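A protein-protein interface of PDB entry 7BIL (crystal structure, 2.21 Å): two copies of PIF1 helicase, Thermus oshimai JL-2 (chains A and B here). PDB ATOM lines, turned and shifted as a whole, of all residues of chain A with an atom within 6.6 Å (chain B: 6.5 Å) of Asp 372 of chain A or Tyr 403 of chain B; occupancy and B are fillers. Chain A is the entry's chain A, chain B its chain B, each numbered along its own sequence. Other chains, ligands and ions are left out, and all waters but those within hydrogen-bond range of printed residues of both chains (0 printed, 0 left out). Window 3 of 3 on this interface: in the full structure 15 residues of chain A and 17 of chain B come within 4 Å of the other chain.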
ATOM      1  N   LEU A 322      -1.841 -25.542  -8.893  1.00  0.00           N
ATOM      2  CA  LEU A 322      -0.984 -25.312 -10.055  1.00  0.00           C
ATOM      3  C   LEU A 322       0.341 -24.748  -9.566  1.00  0.00           C
ATOM      4  O   LEU A 322       0.357 -23.888  -8.679  1.00  0.00           O
ATOM      5  CB  LEU A 322      -1.620 -24.370 -11.092  1.00  0.00           C
ATOM      6  CG  LEU A 322      -0.765 -24.098 -12.341  1.00  0.00           C
ATOM      7  CD1 LEU A 322      -0.525 -25.368 -13.131  1.00  0.00           C
ATOM      8  CD2 LEU A 322      -1.377 -23.061 -13.230  1.00  0.00           C
ATOM      9  N   TYR A 324       3.961 -22.848 -10.288  1.00  0.00           N
ATOM     10  CA  TYR A 324       4.749 -21.931 -11.110  1.00  0.00           C
ATOM     11  C   TYR A 324       6.224 -22.079 -10.736  1.00  0.00           C
ATOM     12  O   TYR A 324       6.629 -21.764  -9.612  1.00  0.00           O
ATOM     13  CB  TYR A 324       4.256 -20.493 -10.946  1.00  0.00           C
ATOM     14  CG  TYR A 324       2.883 -20.309 -11.552  1.00  0.00           C
ATOM     15  CD1 TYR A 324       1.735 -20.575 -10.806  1.00  0.00           C
ATOM     16  CD2 TYR A 324       2.730 -19.913 -12.888  1.00  0.00           C
ATOM     17  CE1 TYR A 324       0.468 -20.437 -11.354  1.00  0.00           C
ATOM     18  CE2 TYR A 324       1.461 -19.777 -13.454  1.00  0.00           C
ATOM     19  CZ  TYR A 324       0.338 -20.038 -12.678  1.00  0.00           C
ATOM     20  OH  TYR A 324      -0.913 -19.926 -13.222  1.00  0.00           O
ATOM     21  N   LYS A 347      -7.232 -21.566  -7.167  1.00  0.00           N
ATOM     22  CA  LYS A 347      -8.261 -20.580  -7.429  1.00  0.00           C
ATOM     23  C   LYS A 347      -8.883 -20.191  -6.096  1.00  0.00           C
ATOM     24  O   LYS A 347      -9.163 -21.051  -5.261  1.00  0.00           O
ATOM     25  CB  LYS A 347      -9.312 -21.151  -8.386  1.00  0.00           C
ATOM     26  CG  LYS A 347     -10.492 -20.230  -8.632  1.00  0.00           C
ATOM     27  CD  LYS A 347     -11.563 -20.864  -9.515  1.00  0.00           C
ATOM     28  CE  LYS A 347     -12.597 -19.815  -9.941  1.00  0.00           C
ATOM     29  NZ  LYS A 347     -13.632 -20.367 -10.863  1.00  0.00           N
ATOM     30  N   TRP A 369      -7.382 -11.866  -5.425  1.00  0.00           N
ATOM     31  CA  TRP A 369      -7.648 -13.299  -5.347  1.00  0.00           C
ATOM     32  C   TRP A 369      -7.461 -13.930  -6.716  1.00  0.00           C
ATOM     33  O   TRP A 369      -7.798 -13.320  -7.731  1.00  0.00           O
ATOM     34  CB  TRP A 369      -9.081 -13.565  -4.861  1.00  0.00           C
ATOM     35  CG  TRP A 369      -9.374 -12.989  -3.499  1.00  0.00           C
ATOM     36  CD1 TRP A 369      -9.257 -13.631  -2.286  1.00  0.00           C
ATOM     37  CD2 TRP A 369      -9.806 -11.656  -3.204  1.00  0.00           C
ATOM     38  NE1 TRP A 369      -9.596 -12.778  -1.261  1.00  0.00           N
ATOM     39  CE2 TRP A 369      -9.938 -11.560  -1.792  1.00  0.00           C
ATOM     40  CE3 TRP A 369     -10.093 -10.535  -3.987  1.00  0.00           C
ATOM     41  CZ2 TRP A 369     -10.354 -10.380  -1.152  1.00  0.00           C
ATOM     42  CZ3 TRP A 369     -10.507  -9.358  -3.349  1.00  0.00           C
ATOM     43  CH2 TRP A 369     -10.637  -9.296  -1.946  1.00  0.00           C
ATOM     44  N   VAL A 370      -6.956 -15.166  -6.737  1.00  0.00           N
ATOM     45  CA  VAL A 370      -6.730 -15.889  -7.986  1.00  0.00           C
ATOM     46  C   VAL A 370      -8.058 -16.345  -8.582  1.00  0.00           C
ATOM     47  O   VAL A 370      -8.889 -16.948  -7.891  1.00  0.00           O
ATOM     48  CB  VAL A 370      -5.806 -17.091  -7.753  1.00  0.00           C
ATOM     49  CG1 VAL A 370      -5.625 -17.855  -9.053  1.00  0.00           C
ATOM     50  CG2 VAL A 370      -4.461 -16.653  -7.148  1.00  0.00           C
ATOM     51  N   GLU A 371      -8.259 -16.078  -9.876  1.00  0.00           N
ATOM     52  CA  GLU A 371      -9.429 -16.556 -10.616  1.00  0.00           C
ATOM     53  C   GLU A 371      -9.113 -17.678 -11.588  1.00  0.00           C
ATOM     54  O   GLU A 371      -9.875 -18.649 -11.680  1.00  0.00           O
ATOM     55  CB  GLU A 371     -10.090 -15.417 -11.395  1.00  0.00           C
ATOM     56  CG  GLU A 371     -10.673 -14.353 -10.527  1.00  0.00           C
ATOM     57  CD  GLU A 371     -11.869 -13.679 -11.162  1.00  0.00           C
ATOM     58  OE1 GLU A 371     -12.055 -13.785 -12.403  1.00  0.00           O
ATOM     59  OE2 GLU A 371     -12.633 -13.052 -10.395  1.00  0.00           O
ATOM     60  N   ASP A 372      -8.032 -17.540 -12.348  1.00  0.00           N
ATOM     61  CA  ASP A 372      -7.616 -18.515 -13.344  1.00  0.00           C
ATOM     62  C   ASP A 372      -6.137 -18.833 -13.170  1.00  0.00           C
ATOM     63  O   ASP A 372      -5.352 -17.991 -12.728  1.00  0.00           O
ATOM     64  CB  ASP A 372      -7.880 -18.015 -14.763  1.00  0.00           C
ATOM     65  CG  ASP A 372      -9.352 -18.077 -15.142  1.00  0.00           C
ATOM     66  OD1 ASP A 372     -10.032 -19.057 -14.758  1.00  0.00           O
ATOM     67  OD2 ASP A 372      -9.821 -17.149 -15.842  1.00  0.00           O
ATOM     68  N   LEU A 373      -5.775 -20.076 -13.470  1.00  0.00           N
ATOM     69  CA  LEU A 373      -4.402 -20.547 -13.342  1.00  0.00           C
ATOM     70  C   LEU A 373      -4.100 -21.320 -14.606  1.00  0.00           C
ATOM     71  O   LEU A 373      -4.765 -22.317 -14.901  1.00  0.00           O
ATOM     72  CB  LEU A 373      -4.222 -21.439 -12.118  1.00  0.00           C
ATOM     73  CG  LEU A 373      -4.287 -20.822 -10.728  1.00  0.00           C
ATOM     74  CD1 LEU A 373      -4.315 -21.950  -9.692  1.00  0.00           C
ATOM     75  CD2 LEU A 373      -3.094 -19.900 -10.507  1.00  0.00           C
ATOM     76  N   GLU A 374      -3.167 -20.806 -15.392  1.00  0.00           N
ATOM     77  CA  GLU A 374      -2.727 -21.432 -16.624  1.00  0.00           C
ATOM     78  C   GLU A 374      -1.206 -21.424 -16.648  1.00  0.00           C
ATOM     79  O   GLU A 374      -0.561 -20.821 -15.784  1.00  0.00           O
ATOM     80  CB  GLU A 374      -3.336 -20.743 -17.845  1.00  0.00           C
ATOM     81  CG  GLU A 374      -4.860 -20.648 -17.776  1.00  0.00           C
ATOM     82  CD  GLU A 374      -5.582 -22.010 -17.732  1.00  0.00           C
ATOM     83  OE1 GLU A 374      -5.027 -23.048 -18.176  1.00  0.00           O
ATOM     84  OE2 GLU A 374      -6.738 -22.034 -17.248  1.00  0.00           O
ATOM     85  N   ALA A 377       0.518 -17.909 -16.945  1.00  0.00           N
ATOM     86  CA  ALA A 377      -0.385 -16.781 -16.865  1.00  0.00           C
ATOM     87  C   ALA A 377      -1.470 -17.103 -15.848  1.00  0.00           C
ATOM     88  O   ALA A 377      -1.995 -18.218 -15.830  1.00  0.00           O
ATOM     89  CB  ALA A 377      -0.998 -16.510 -18.252  1.00  0.00           C
ATOM     90  N   LEU A 378      -1.826 -16.119 -15.034  1.00  0.00           N
ATOM     91  CA  LEU A 378      -2.941 -16.241 -14.124  1.00  0.00           C
ATOM     92  C   LEU A 378      -3.743 -14.951 -14.158  1.00  0.00           C
ATOM     93  O   LEU A 378      -3.247 -13.886 -14.549  1.00  0.00           O
ATOM     94  CB  LEU A 378      -2.493 -16.575 -12.694  1.00  0.00           C
ATOM     95  CG  LEU A 378      -1.473 -15.674 -12.019  1.00  0.00           C
ATOM     96  CD1 LEU A 378      -1.702 -15.657 -10.517  1.00  0.00           C
ATOM     97  CD2 LEU A 378      -0.105 -16.187 -12.323  1.00  0.00           C
ATOM     98  N   ALA A 379      -4.994 -15.053 -13.734  1.00  0.00           N
ATOM     99  CA  ALA A 379      -5.888 -13.912 -13.646  1.00  0.00           C
ATOM    100  C   ALA A 379      -6.174 -13.666 -12.180  1.00  0.00           C
ATOM    101  O   ALA A 379      -6.488 -14.601 -11.432  1.00  0.00           O
ATOM    102  CB  ALA A 379      -7.192 -14.158 -14.401  1.00  0.00           C
ATOM    103  N   VAL A 380      -6.033 -12.419 -11.769  1.00  0.00           N
ATOM    104  CA  VAL A 380      -6.251 -12.016 -10.389  1.00  0.00           C
ATOM    105  C   VAL A 380      -7.349 -10.961 -10.364  1.00  0.00           C
ATOM    106  O   VAL A 380      -7.411 -10.088 -11.243  1.00  0.00           O
ATOM    107  CB  VAL A 380      -4.937 -11.500  -9.779  1.00  0.00           C
ATOM    108  CG1 VAL A 380      -5.167 -10.901  -8.436  1.00  0.00           C
ATOM    109  CG2 VAL A 380      -3.896 -12.634  -9.724  1.00  0.00           C
ATOM    110  N   ARG A 381      -8.256 -11.090  -9.399  1.00  0.00           N
ATOM    111  CA  ARG A 381      -9.330 -10.130  -9.185  1.00  0.00           C
ATOM    112  C   ARG A 381      -8.846  -9.156  -8.120  1.00  0.00           C
ATOM    113  O   ARG A 381      -8.587  -9.567  -6.985  1.00  0.00           O
ATOM    114  CB  ARG A 381     -10.609 -10.859  -8.749  1.00  0.00           C
ATOM    115  CG  ARG A 381     -11.881 -10.003  -8.560  1.00  0.00           C
ATOM    116  CD  ARG A 381     -12.391  -9.308  -9.829  1.00  0.00           C
ATOM    117  NE  ARG A 381     -12.892 -10.240 -10.839  1.00  0.00           N
ATOM    118  CZ  ARG A 381     -13.501  -9.874 -11.968  1.00  0.00           C
ATOM    119  NH1 ARG A 381     -13.703  -8.590 -12.232  1.00  0.00           N
ATOM    120  NH2 ARG A 381     -13.912 -10.789 -12.844  1.00  0.00           N
ATOM    121  N   ARG A 388     -10.215  -7.466 -13.165  1.00  0.00           N
ATOM    122  CA  ARG A 388      -9.494  -8.697 -13.437  1.00  0.00           C
ATOM    123  C   ARG A 388      -8.262  -8.365 -14.274  1.00  0.00           C
ATOM    124  O   ARG A 388      -8.375  -7.704 -15.315  1.00  0.00           O
ATOM    125  CB  ARG A 388     -10.426  -9.651 -14.174  1.00  0.00           C
ATOM    126  CG  ARG A 388      -9.812 -10.874 -14.712  1.00  0.00           C
ATOM    127  CD  ARG A 388     -10.894 -11.662 -15.371  1.00  0.00           C
ATOM    128  NE  ARG A 388     -10.328 -12.560 -16.358  1.00  0.00           N
ATOM    129  CZ  ARG A 388     -10.308 -13.878 -16.237  1.00  0.00           C
ATOM    130  NH1 ARG A 388     -10.847 -14.450 -15.170  1.00  0.00           N
ATOM    131  NH2 ARG A 388      -9.770 -14.616 -17.196  1.00  0.00           N
ATOM    132  N   GLU B 221      -5.768 -10.567 -21.540  1.00  0.00           N
ATOM    133  CA  GLU B 221      -6.557 -11.787 -21.739  1.00  0.00           C
ATOM    134  C   GLU B 221      -6.079 -12.629 -22.917  1.00  0.00           C
ATOM    135  O   GLU B 221      -6.330 -13.847 -22.958  1.00  0.00           O
ATOM    136  CB  GLU B 221      -8.029 -11.413 -21.891  1.00  0.00           C
ATOM    137  CG  GLU B 221      -8.597 -10.687 -20.655  1.00  0.00           C
ATOM    138  CD  GLU B 221      -8.858 -11.636 -19.483  1.00  0.00           C
ATOM    139  OE1 GLU B 221      -9.128 -11.161 -18.356  1.00  0.00           O
ATOM    140  OE2 GLU B 221      -8.803 -12.864 -19.696  1.00  0.00           O
ATOM    141  N   LEU B 224      -3.553 -15.032 -21.719  1.00  0.00           N
ATOM    142  CA  LEU B 224      -4.183 -16.062 -20.896  1.00  0.00           C
ATOM    143  C   LEU B 224      -4.886 -17.089 -21.762  1.00  0.00           C
ATOM    144  O   LEU B 224      -4.854 -18.286 -21.456  1.00  0.00           O
ATOM    145  CB  LEU B 224      -5.195 -15.443 -19.925  1.00  0.00           C
ATOM    146  CG  LEU B 224      -5.829 -16.396 -18.905  1.00  0.00           C
ATOM    147  CD1 LEU B 224      -4.807 -16.810 -17.894  1.00  0.00           C
ATOM    148  CD2 LEU B 224      -6.995 -15.767 -18.194  1.00  0.00           C
ATOM    149  N   ARG B 228      -4.216 -21.151 -21.848  1.00  0.00           N
ATOM    150  CA  ARG B 228      -5.289 -22.089 -21.527  1.00  0.00           C
ATOM    151  C   ARG B 228      -5.546 -23.030 -22.699  1.00  0.00           C
ATOM    152  O   ARG B 228      -5.838 -24.214 -22.495  1.00  0.00           O
ATOM    153  CB  ARG B 228      -6.562 -21.325 -21.136  1.00  0.00           C
ATOM    154  CG  ARG B 228      -7.852 -22.147 -21.081  1.00  0.00           C
ATOM    155  CD  ARG B 228      -9.090 -21.312 -20.646  1.00  0.00           C
ATOM    156  NE  ARG B 228      -9.213 -20.027 -21.344  1.00  0.00           N
ATOM    157  CZ  ARG B 228      -9.089 -18.830 -20.763  1.00  0.00           C
ATOM    158  NH1 ARG B 228      -8.853 -18.747 -19.445  1.00  0.00           N
ATOM    159  NH2 ARG B 228      -9.213 -17.714 -21.492  1.00  0.00           N
ATOM    160  N   TYR B 401      -9.511  -7.118 -25.622  1.00  0.00           N
ATOM    161  CA  TYR B 401     -10.223  -8.362 -25.314  1.00  0.00           C
ATOM    162  C   TYR B 401     -10.827  -8.322 -23.908  1.00  0.00           C
ATOM    163  O   TYR B 401     -10.127  -8.030 -22.936  1.00  0.00           O
ATOM    164  CB  TYR B 401      -9.308  -9.577 -25.467  1.00  0.00           C
ATOM    165  CG  TYR B 401      -8.573  -9.607 -26.772  1.00  0.00           C
ATOM    166  CD1 TYR B 401      -7.370  -8.916 -26.919  1.00  0.00           C
ATOM    167  CD2 TYR B 401      -9.080 -10.309 -27.875  1.00  0.00           C
ATOM    168  CE1 TYR B 401      -6.678  -8.915 -28.128  1.00  0.00           C
ATOM    169  CE2 TYR B 401      -8.390 -10.315 -29.111  1.00  0.00           C
ATOM    170  CZ  TYR B 401      -7.188  -9.612 -29.223  1.00  0.00           C
ATOM    171  OH  TYR B 401      -6.474  -9.605 -30.410  1.00  0.00           O
ATOM    172  N   THR B 402     -12.131  -8.608 -23.806  1.00  0.00           N
ATOM    173  CA  THR B 402     -12.990  -8.340 -22.651  1.00  0.00           C
ATOM    174  C   THR B 402     -13.204  -9.523 -21.690  1.00  0.00           C
ATOM    175  O   THR B 402     -13.271  -9.267 -20.476  1.00  0.00           O
ATOM    176  CB  THR B 402     -14.328  -7.706 -23.041  1.00  0.00           C
ATOM    177  OG1 THR B 402     -14.774  -8.182 -24.309  1.00  0.00           O
ATOM    178  CG2 THR B 402     -14.155  -6.189 -23.064  1.00  0.00           C
ATOM    179  N   TYR B 403     -13.269 -10.804 -22.106  1.00  0.00           N
ATOM    180  CA  TYR B 403     -13.492 -11.866 -21.084  1.00  0.00           C
ATOM    181  C   TYR B 403     -14.756 -11.822 -20.199  1.00  0.00           C
ATOM    182  O   TYR B 403     -14.677 -11.531 -19.012  1.00  0.00           O
ATOM    183  CB  TYR B 403     -12.296 -12.107 -20.169  1.00  0.00           C
ATOM    184  CG  TYR B 403     -12.370 -13.548 -19.662  1.00  0.00           C
ATOM    185  CD1 TYR B 403     -11.773 -14.585 -20.382  1.00  0.00           C
ATOM    186  CD2 TYR B 403     -13.111 -13.882 -18.528  1.00  0.00           C
ATOM    187  CE1 TYR B 403     -11.863 -15.899 -19.961  1.00  0.00           C
ATOM    188  CE2 TYR B 403     -13.219 -15.203 -18.096  1.00  0.00           C
ATOM    189  CZ  TYR B 403     -12.582 -16.207 -18.822  1.00  0.00           C
ATOM    190  OH  TYR B 403     -12.663 -17.523 -18.412  1.00  0.00           O
ATOM    191  N   ASP B 404     -15.933 -11.938 -20.815  1.00  0.00           N
ATOM    192  CA  ASP B 404     -17.187 -11.884 -20.055  1.00  0.00           C
ATOM    193  C   ASP B 404     -17.194 -12.945 -18.950  1.00  0.00           C
ATOM    194  O   ASP B 404     -16.710 -14.065 -19.116  1.00  0.00           O
ATOM    195  CB  ASP B 404     -18.363 -12.387 -20.924  1.00  0.00           C
ATOM    196  CG  ASP B 404     -18.984 -11.388 -21.845  1.00  0.00           C
ATOM    197  OD1 ASP B 404     -18.365 -11.040 -22.881  1.00  0.00           O
ATOM    198  OD2 ASP B 404     -20.157 -11.037 -21.570  1.00  0.00           O
ATOM    199  N   SER B 405     -17.670 -12.517 -17.773  1.00  0.00           N
ATOM    200  CA  SER B 405     -17.554 -13.243 -16.510  1.00  0.00           C
ATOM    201  C   SER B 405     -18.544 -14.402 -16.415  1.00  0.00           C
ATOM    202  O   SER B 405     -18.164 -15.526 -16.070  1.00  0.00           O
ATOM    203  CB  SER B 405     -17.751 -12.268 -15.347  1.00  0.00           C
ATOM    204  OG  SER B 405     -16.901 -11.143 -15.493  1.00  0.00           O
ATOM    205  N   GLU B 406     -19.816 -14.153 -16.761  1.00  0.00           N
ATOM    206  CA  GLU B 406     -20.851 -15.187 -16.679  1.00  0.00           C
ATOM    207  C   GLU B 406     -20.580 -16.291 -17.698  1.00  0.00           C
ATOM    208  O   GLU B 406     -20.861 -17.466 -17.438  1.00  0.00           O
ATOM    209  CB  GLU B 406     -22.246 -14.585 -16.896  1.00  0.00           C
ATOM    210  CG  GLU B 406     -22.829 -13.766 -15.728  1.00  0.00           C
ATOM    211  CD  GLU B 406     -23.146 -14.599 -14.485  1.00  0.00           C
ATOM    212  OE1 GLU B 406     -22.191 -15.040 -13.802  1.00  0.00           O
ATOM    213  OE2 GLU B 406     -24.348 -14.807 -14.181  1.00  0.00           O
ATOM    214  N   ARG B 407     -20.045 -15.929 -18.857  1.00  0.00           N
ATOM    215  CA  ARG B 407     -19.707 -16.848 -19.931  1.00  0.00           C
ATOM    216  C   ARG B 407     -18.224 -17.186 -19.812  1.00  0.00           C
ATOM    217  O   ARG B 407     -17.442 -16.445 -19.214  1.00  0.00           O
ATOM    218  CB  ARG B 407     -20.003 -16.251 -21.317  1.00  0.00           C
ATOM    219  CG  ARG B 407     -21.438 -15.777 -21.584  1.00  0.00           C
ATOM    220  CD  ARG B 407     -22.440 -16.927 -21.727  1.00  0.00           C
ATOM    221  NE  ARG B 407     -23.103 -17.236 -20.449  1.00  0.00           N
ATOM    222  CZ  ARG B 407     -24.098 -18.113 -20.279  1.00  0.00           C
ATOM    223  NH1 ARG B 407     -24.579 -18.797 -21.311  1.00  0.00           N
ATOM    224  NH2 ARG B 407     -24.619 -18.309 -19.075  1.00  0.00           N
ATOM    225  N   GLU B 408     -17.852 -18.352 -20.303  1.00  0.00           N
ATOM    226  CA  GLU B 408     -16.477 -18.814 -20.186  1.00  0.00           C
ATOM    227  C   GLU B 408     -15.585 -18.229 -21.277  1.00  0.00           C
ATOM    228  O   GLU B 408     -14.479 -18.731 -21.513  1.00  0.00           O
ATOM    229  CB  GLU B 408     -16.443 -20.346 -20.255  1.00  0.00           C
ATOM    230  CG  GLU B 408     -16.903 -20.912 -21.618  1.00  0.00           C
ATOM    231  CD  GLU B 408     -17.418 -22.353 -21.553  1.00  0.00           C
ATOM    232  OE1 GLU B 408     -18.087 -22.774 -22.526  1.00  0.00           O
ATOM    233  OE2 GLU B 408     -17.160 -23.055 -20.543  1.00  0.00           O
ATOM    234  N   GLU B 409     -16.056 -17.185 -21.961  1.00  0.00           N
ATOM    235  CA  GLU B 409     -15.516 -16.788 -23.253  1.00  0.00           C
ATOM    236  C   GLU B 409     -14.885 -15.395 -23.247  1.00  0.00           C
ATOM    237  O   GLU B 409     -15.235 -14.519 -22.449  1.00  0.00           O
ATOM    238  CB  GLU B 409     -16.630 -16.866 -24.324  1.00  0.00           C
ATOM    239  CG  GLU B 409     -17.066 -18.313 -24.629  1.00  0.00           C
ATOM    240  CD  GLU B 409     -18.575 -18.500 -24.698  1.00  0.00           C
ATOM    241  OE1 GLU B 409     -19.224 -17.790 -25.505  1.00  0.00           O
ATOM    242  OE2 GLU B 409     -19.104 -19.358 -23.941  1.00  0.00           O
ATOM    243  N   ILE B 410     -13.961 -15.212 -24.180  1.00  0.00           N
ATOM    244  CA  ILE B 410     -13.262 -13.962 -24.452  1.00  0.00           C
ATOM    245  C   ILE B 410     -13.810 -13.400 -25.757  1.00  0.00           C
ATOM    246  O   ILE B 410     -14.184 -14.157 -26.664  1.00  0.00           O
ATOM    247  CB  ILE B 410     -11.734 -14.187 -24.507  1.00  0.00           C
ATOM    248  CG1 ILE B 410     -10.977 -12.903 -24.780  1.00  0.00           C
ATOM    249  CG2 ILE B 410     -11.353 -15.185 -25.575  1.00  0.00           C
ATOM    250  CD1 ILE B 410      -9.504 -13.157 -25.033  1.00  0.00           C
ATOM    251  N   LYS B 411     -13.892 -12.065 -25.847  1.00  0.00           N
ATOM    252  CA  LYS B 411     -14.416 -11.414 -27.069  1.00  0.00           C
ATOM    253  C   LYS B 411     -13.602 -10.176 -27.448  1.00  0.00           C
ATOM    254  O   LYS B 411     -13.250  -9.370 -26.570  1.00  0.00           O
ATOM    255  CB  LYS B 411     -15.895 -11.028 -26.911  1.00  0.00           C
ATOM    256  CG  LYS B 411     -16.867 -12.114 -27.365  1.00  0.00           C
ATOM    257  CD  LYS B 411     -18.323 -11.636 -27.397  1.00  0.00           C
ATOM    258  CE  LYS B 411     -18.650 -10.907 -28.709  1.00  0.00           C
ATOM    259  NZ  LYS B 411     -20.127 -10.877 -28.925  1.00  0.00           N
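NE of Arg 388 of chain A lies within salt-bridge range of OE1 of Glu 221 of chain B.
OH of Tyr 324 of chain A is in hydrogen-bond range of O of Glu 374 of chain A (2.7 Å). OD2 of Asp 372 of chain A lies within salt-bridge range of NH2 of Arg 388 of chain A. The backbone carbonyl oxygen of Ala 377 of chain A is in hydrogen-bond range of the side-chain hydroxyl of Tyr 324 of chain A (3.3 Å). The guanidinium group of Arg 388 of chain A lies within salt-bridge range of the side-chain carboxylate of Glu 371 of chain A. The backbone NH (N) of Ala 379 of chain A is in hydrogen-bond range of the backbone carbonyl oxygen (O) of Asp 372 of chain A, at 3.1 Å.
Among the printed residues, pairs that only touch across the chains: Arg 388 of chain A with Leu 224 of chain B, Glu 374 of chain A with Arg 228 of chain B, Arg 388 of chain A with Tyr 403 of chain B, Ala 377 of chain A with Leu 224 of chain B, Glu 374 of chain A with Leu 224 of chain B, Asp 372 of chain A with Tyr 403 of chain B and Asp 372 of chain A with Leu 224 of chain B.
Of chain B, only Leu 224 and Tyr 403 come within 4 Å of Asp 372 of chain A. Printed residues of chain B within 4 Å of Ala 377 of chain A: Leu 224. Of the printed residues of chain B, Arg 388 of chain A touches Glu 221, Leu 224 and Tyr 403. Of the printed residues of chain A, Glu 221 of chain B touches Arg 388. Printed residues of chain A within 4 Å of Leu 224 of chain B: Asp 372, Glu 374, Ala 377 and Arg 388. The nearest residue of chain B that does not touch Asp 372 of chain A is Arg 228 of chain B (4.1 Å). The nearest residue of chain A that does not touch Tyr 403 of chain B is Glu 371 of chain A (6.0 Å).
Printed residues of chain B that touch a printed residue of chain A: Glu 221, Leu 224, Arg 228 and Tyr 403. Of the 15 printed residues of chain A, 4 touch a printed residue of chain B. Among the printed residues, Asp or Glu carboxylates within 4 Å of a Lys or Arg side-chain nitrogen of the other chain: Arg 388 of chain A with Glu 221 of chain B (2.7 Å).
No position is printed for both chains. Of the 8 pairs that touch across the chains among the printed residues, none has its exchanged pair printed and touching as well.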
